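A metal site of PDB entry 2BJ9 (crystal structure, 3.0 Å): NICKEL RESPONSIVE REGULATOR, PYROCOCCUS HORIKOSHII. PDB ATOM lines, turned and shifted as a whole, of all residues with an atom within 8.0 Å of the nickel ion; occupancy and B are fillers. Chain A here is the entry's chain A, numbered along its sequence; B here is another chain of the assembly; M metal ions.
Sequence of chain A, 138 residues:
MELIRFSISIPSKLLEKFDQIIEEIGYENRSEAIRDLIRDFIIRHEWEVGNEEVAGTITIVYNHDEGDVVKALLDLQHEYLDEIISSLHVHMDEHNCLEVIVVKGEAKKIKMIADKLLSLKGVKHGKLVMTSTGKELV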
ATOM      1  N   ASN A  63     -22.377  12.956  -5.356  1.00  0.00           N
ATOM      2  CA  ASN A  63     -21.994  12.582  -6.707  1.00  0.00           C
ATOM      3  C   ASN A  63     -22.445  11.143  -6.831  1.00  0.00           C
ATOM      4  O   ASN A  63     -21.833  10.264  -6.241  1.00  0.00           O
ATOM      5  CB  ASN A  63     -20.480  12.635  -6.858  1.00  0.00           C
ATOM      6  CG  ASN A  63     -20.028  12.347  -8.262  1.00  0.00           C
ATOM      7  OD1 ASN A  63     -20.596  11.491  -8.940  1.00  0.00           O
ATOM      8  ND2 ASN A  63     -18.996  13.057  -8.706  1.00  0.00           N
ATOM      9  N   HIS A  64     -23.493  10.887  -7.609  1.00  0.00           N
ATOM     10  CA  HIS A  64     -23.990   9.521  -7.726  1.00  0.00           C
ATOM     11  C   HIS A  64     -22.994   8.592  -8.393  1.00  0.00           C
ATOM     12  O   HIS A  64     -23.108   7.375  -8.298  1.00  0.00           O
ATOM     13  CB  HIS A  64     -25.313   9.476  -8.480  1.00  0.00           C
ATOM     14  CG  HIS A  64     -25.175   9.698  -9.951  1.00  0.00           C
ATOM     15  ND1 HIS A  64     -25.187  10.956 -10.523  1.00  0.00           N
ATOM     16  CD2 HIS A  64     -25.005   8.820 -10.966  1.00  0.00           C
ATOM     17  CE1 HIS A  64     -25.025  10.839 -11.830  1.00  0.00           C
ATOM     18  NE2 HIS A  64     -24.911   9.553 -12.124  1.00  0.00           N
ATOM     19  N   ASP A  65     -22.020   9.164  -9.089  1.00  0.00           N
ATOM     20  CA  ASP A  65     -21.029   8.351  -9.756  1.00  0.00           C
ATOM     21  C   ASP A  65     -19.807   8.097  -8.906  1.00  0.00           C
ATOM     22  O   ASP A  65     -18.896   7.396  -9.333  1.00  0.00           O
ATOM     23  CB  ASP A  65     -20.598   9.001 -11.074  1.00  0.00           C
ATOM     24  CG  ASP A  65     -21.692   8.981 -12.129  1.00  0.00           C
ATOM     25  OD1 ASP A  65     -22.335   7.910 -12.303  1.00  0.00           O
ATOM     26  OD2 ASP A  65     -21.898  10.019 -12.796  1.00  0.00           O
ATOM     27  N   GLU A  66     -19.782   8.641  -7.692  1.00  0.00           N
ATOM     28  CA  GLU A  66     -18.637   8.421  -6.822  1.00  0.00           C
ATOM     29  C   GLU A  66     -18.786   7.185  -5.960  1.00  0.00           C
ATOM     30  O   GLU A  66     -19.874   6.905  -5.463  1.00  0.00           O
ATOM     31  CB  GLU A  66     -18.390   9.624  -5.910  1.00  0.00           C
ATOM     32  CG  GLU A  66     -17.166   9.418  -5.028  1.00  0.00           C
ATOM     33  CD  GLU A  66     -16.764  10.648  -4.272  1.00  0.00           C
ATOM     34  OE1 GLU A  66     -16.739  11.744  -4.886  1.00  0.00           O
ATOM     35  OE2 GLU A  66     -16.454  10.532  -3.060  1.00  0.00           O
ATOM     36  N   VAL A  70     -24.455   5.728  -3.844  1.00  0.00           N
ATOM     37  CA  VAL A  70     -25.840   5.517  -4.239  1.00  0.00           C
ATOM     38  C   VAL A  70     -26.476   4.320  -3.549  1.00  0.00           C
ATOM     39  O   VAL A  70     -27.575   4.427  -3.011  1.00  0.00           O
ATOM     40  CB  VAL A  70     -25.981   5.338  -5.758  1.00  0.00           C
ATOM     41  CG1 VAL A  70     -27.443   5.197  -6.126  1.00  0.00           C
ATOM     42  CG2 VAL A  70     -25.368   6.528  -6.482  1.00  0.00           C
ATOM     43  N   ASP A  93     -26.834  17.976 -12.000  1.00  0.00           N
ATOM     44  CA  ASP A  93     -26.041  17.991 -13.233  1.00  0.00           C
ATOM     45  C   ASP A  93     -25.576  16.586 -13.606  1.00  0.00           C
ATOM     46  O   ASP A  93     -26.072  15.598 -13.065  1.00  0.00           O
ATOM     47  CB  ASP A  93     -24.837  18.936 -13.131  1.00  0.00           C
ATOM     48  CG  ASP A  93     -23.809  18.508 -12.090  1.00  0.00           C
ATOM     49  OD1 ASP A  93     -23.408  17.333 -12.091  1.00  0.00           O
ATOM     50  OD2 ASP A  93     -23.400  19.375 -11.283  1.00  0.00           O
ATOM     51  N   GLU A  94     -24.629  16.488 -14.525  1.00  0.00           N
ATOM     52  CA  GLU A  94     -24.171  15.174 -14.951  1.00  0.00           C
ATOM     53  C   GLU A  94     -23.863  14.222 -13.803  1.00  0.00           C
ATOM     54  O   GLU A  94     -24.258  13.049 -13.855  1.00  0.00           O
ATOM     55  CB  GLU A  94     -22.943  15.314 -15.852  1.00  0.00           C
ATOM     56  CG  GLU A  94     -22.527  14.018 -16.536  1.00  0.00           C
ATOM     57  CD  GLU A  94     -21.391  14.224 -17.535  1.00  0.00           C
ATOM     58  OE1 GLU A  94     -21.010  13.235 -18.200  1.00  0.00           O
ATOM     59  OE2 GLU A  94     -20.875  15.359 -17.652  1.00  0.00           O
ATOM     60  N   HIS A  95     -23.204  14.706 -12.769  1.00  0.00           N
ATOM     61  CA  HIS A  95     -22.821  13.850 -11.641  1.00  0.00           C
ATOM     62  C   HIS A  95     -23.529  14.074 -10.324  1.00  0.00           C
ATOM     63  O   HIS A  95     -23.834  13.133  -9.597  1.00  0.00           O
ATOM     64  CB  HIS A  95     -21.310  13.984 -11.390  1.00  0.00           C
ATOM     65  CG  HIS A  95     -20.451  13.580 -12.549  1.00  0.00           C
ATOM     66  ND1 HIS A  95     -20.293  12.263 -12.924  1.00  0.00           N
ATOM     67  CD2 HIS A  95     -19.714  14.312 -13.411  1.00  0.00           C
ATOM     68  CE1 HIS A  95     -19.481  12.212 -13.977  1.00  0.00           C
ATOM     69  NE2 HIS A  95     -19.114  13.443 -14.282  1.00  0.00           N
ATOM     70  N   ASN A  96     -23.782  15.339 -10.005  1.00  0.00           N
ATOM     71  CA  ASN A  96     -24.384  15.691  -8.733  1.00  0.00           C
ATOM     72  C   ASN A  96     -25.897  15.608  -8.575  1.00  0.00           C
ATOM     73  O   ASN A  96     -26.652  15.979  -9.478  1.00  0.00           O
ATOM     74  CB  ASN A  96     -23.890  17.082  -8.343  1.00  0.00           C
ATOM     75  CG  ASN A  96     -22.375  17.162  -8.357  1.00  0.00           C
ATOM     76  OD1 ASN A  96     -21.688  16.475  -7.613  1.00  0.00           O
ATOM     77  ND2 ASN A  96     -21.841  18.009  -9.225  1.00  0.00           N
ATOM     78  N   CYS A  97     -26.324  15.119  -7.423  1.00  0.00           N
ATOM     79  CA  CYS A  97     -27.739  14.992  -7.085  1.00  0.00           C
ATOM     80  C   CYS A  97     -27.986  15.705  -5.772  1.00  0.00           C
ATOM     81  O   CYS A  97     -27.070  15.881  -4.973  1.00  0.00           O
ATOM     82  CB  CYS A  97     -28.128  13.520  -6.882  1.00  0.00           C
ATOM     83  SG  CYS A  97     -27.857  12.391  -8.260  1.00  0.00           S
ATOM     84  N   LYS B  71     -28.271   2.342 -10.501  1.00  0.00           N
ATOM     85  CA  LYS B  71     -27.354   3.233 -11.200  1.00  0.00           C
ATOM     86  C   LYS B  71     -27.863   3.483 -12.608  1.00  0.00           C
ATOM     87  O   LYS B  71     -27.928   4.626 -13.058  1.00  0.00           O
ATOM     88  CB  LYS B  71     -25.958   2.618 -11.262  1.00  0.00           C
ATOM     89  CG  LYS B  71     -24.875   3.586 -11.716  1.00  0.00           C
ATOM     90  CD  LYS B  71     -23.543   2.884 -11.921  1.00  0.00           C
ATOM     91  CE  LYS B  71     -22.418   3.894 -12.154  1.00  0.00           C
ATOM     92  NZ  LYS B  71     -22.673   4.774 -13.324  1.00  0.00           N
ATOM     93  N   ALA B  72     -28.222   2.413 -13.303  1.00  0.00           N
ATOM     94  CA  ALA B  72     -28.735   2.517 -14.663  1.00  0.00           C
ATOM     95  C   ALA B  72     -29.796   3.624 -14.741  1.00  0.00           C
ATOM     96  O   ALA B  72     -29.771   4.472 -15.628  1.00  0.00           O
ATOM     97  CB  ALA B  72     -29.339   1.191 -15.102  1.00  0.00           C
ATOM     98  N   LEU B  73     -30.725   3.623 -13.791  1.00  0.00           N
ATOM     99  CA  LEU B  73     -31.766   4.625 -13.756  1.00  0.00           C
ATOM    100  C   LEU B  73     -31.215   6.033 -13.629  1.00  0.00           C
ATOM    101  O   LEU B  73     -31.582   6.904 -14.403  1.00  0.00           O
ATOM    102  CB  LEU B  73     -32.737   4.345 -12.611  1.00  0.00           C
ATOM    103  CG  LEU B  73     -33.814   3.290 -12.888  1.00  0.00           C
ATOM    104  CD1 LEU B  73     -34.571   2.950 -11.616  1.00  0.00           C
ATOM    105  CD2 LEU B  73     -34.757   3.841 -13.937  1.00  0.00           C
ATOM    106  N   LEU B  74     -30.340   6.269 -12.660  1.00  0.00           N
ATOM    107  CA  LEU B  74     -29.769   7.603 -12.476  1.00  0.00           C
ATOM    108  C   LEU B  74     -29.076   8.119 -13.734  1.00  0.00           C
ATOM    109  O   LEU B  74     -29.347   9.224 -14.179  1.00  0.00           O
ATOM    110  CB  LEU B  74     -28.802   7.622 -11.303  1.00  0.00           C
ATOM    111  CG  LEU B  74     -29.437   7.527  -9.921  1.00  0.00           C
ATOM    112  CD1 LEU B  74     -28.359   7.385  -8.873  1.00  0.00           C
ATOM    113  CD2 LEU B  74     -30.286   8.761  -9.655  1.00  0.00           C
ATOM    114  N   ASP B  75     -28.172   7.320 -14.294  1.00  0.00           N
ATOM    115  CA  ASP B  75     -27.461   7.714 -15.503  1.00  0.00           C
ATOM    116  C   ASP B  75     -28.482   8.148 -16.546  1.00  0.00           C
ATOM    117  O   ASP B  75     -28.399   9.257 -17.075  1.00  0.00           O
ATOM    118  CB  ASP B  75     -26.645   6.549 -16.060  1.00  0.00           C
ATOM    119  CG  ASP B  75     -25.535   6.100 -15.124  1.00  0.00           C
ATOM    120  OD1 ASP B  75     -24.882   5.082 -15.429  1.00  0.00           O
ATOM    121  OD2 ASP B  75     -25.306   6.780 -14.090  1.00  0.00           O
ATOM    122  N   LEU B  76     -29.445   7.276 -16.839  1.00  0.00           N
ATOM    123  CA  LEU B  76     -30.495   7.595 -17.801  1.00  0.00           C
ATOM    124  C   LEU B  76     -31.141   8.932 -17.456  1.00  0.00           C
ATOM    125  O   LEU B  76     -31.227   9.824 -18.287  1.00  0.00           O
ATOM    126  CB  LEU B  76     -31.570   6.527 -17.804  1.00  0.00           C
ATOM    127  CG  LEU B  76     -31.334   5.311 -18.682  1.00  0.00           C
ATOM    128  CD1 LEU B  76     -32.567   4.420 -18.659  1.00  0.00           C
ATOM    129  CD2 LEU B  76     -31.044   5.777 -20.098  1.00  0.00           C
ATOM    130  N   HIS B  78     -30.059  11.335 -15.482  1.00  0.00           N
ATOM    131  CA  HIS B  78     -29.130  12.461 -15.555  1.00  0.00           C
ATOM    132  C   HIS B  78     -28.782  12.818 -16.993  1.00  0.00           C
ATOM    133  O   HIS B  78     -28.161  13.858 -17.243  1.00  0.00           O
ATOM    134  CB  HIS B  78     -27.855  12.166 -14.759  1.00  0.00           C
ATOM    135  CG  HIS B  78     -27.999  12.384 -13.289  1.00  0.00           C
ATOM    136  ND1 HIS B  78     -27.466  13.470 -12.643  1.00  0.00           N
ATOM    137  CD2 HIS B  78     -28.675  11.678 -12.340  1.00  0.00           C
ATOM    138  CE1 HIS B  78     -27.795  13.437 -11.365  1.00  0.00           C
ATOM    139  NE2 HIS B  78     -28.527  12.354 -11.158  1.00  0.00           N
ATOM    140  N   GLU B  79     -29.172  11.972 -17.929  1.00  0.00           N
ATOM    141  CA  GLU B  79     -28.908  12.219 -19.332  1.00  0.00           C
ATOM    142  C   GLU B  79     -29.975  13.185 -19.853  1.00  0.00           C
ATOM    143  O   GLU B  79     -29.861  13.738 -20.948  1.00  0.00           O
ATOM    144  CB  GLU B  79     -28.942  10.913 -20.111  1.00  0.00           C
ATOM    145  CG  GLU B  79     -28.647  11.059 -21.601  1.00  0.00           C
ATOM    146  CD  GLU B  79     -28.856   9.761 -22.375  1.00  0.00           C
ATOM    147  OE1 GLU B  79     -28.768   9.796 -23.618  1.00  0.00           O
ATOM    148  OE2 GLU B  79     -29.113   8.711 -21.747  1.00  0.00           O
HETATM  149 NI    NI M   1     -23.723   8.534 -13.726  1.00  0.00          NI
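OD1 of Asn 63 lies within hydrogen-bond range of N of Asp 65 (2.7 Å).
NZ of Lys 71 of chain B is in salt-bridge range of OD1 of Asp 75 of chain B (3.1 Å).
The side-chain sulfur of Cys 97 lies close to a ring nitrogen (ND1) of His 64, at 3.8 Å.
The side-chain carboxylate (OD1) of Asp 65 sits close to the side-chain amino group (NZ) of Lys 71 of chain B, 3.3 Å away.
The backbone carbonyl oxygen (O) of His 95 is in hydrogen-bond range of a ring nitrogen (ND1) of His 64 (2.7 Å).
ND1 of His 95 sits close to OD2 of Asp 65 (2.8 Å).
Lys 71 of chain B touches the nickel ion.
Of the 18 residues printed, 4 come within 4 Å of the nickel ion.
The nickel ion is bound by the side-chain carboxylate (OD1) of Asp 65 (2.1 Å), a ring nitrogen (NE2) of His 64 (2.2 Å), the side-chain carboxylate (OD2) of Asp 75 of chain B (2.4 Å) and the side-chain carboxylate (OD2) of Asp 65 (2.5 Å).
The nickel ion has four donor atoms within binding distance.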
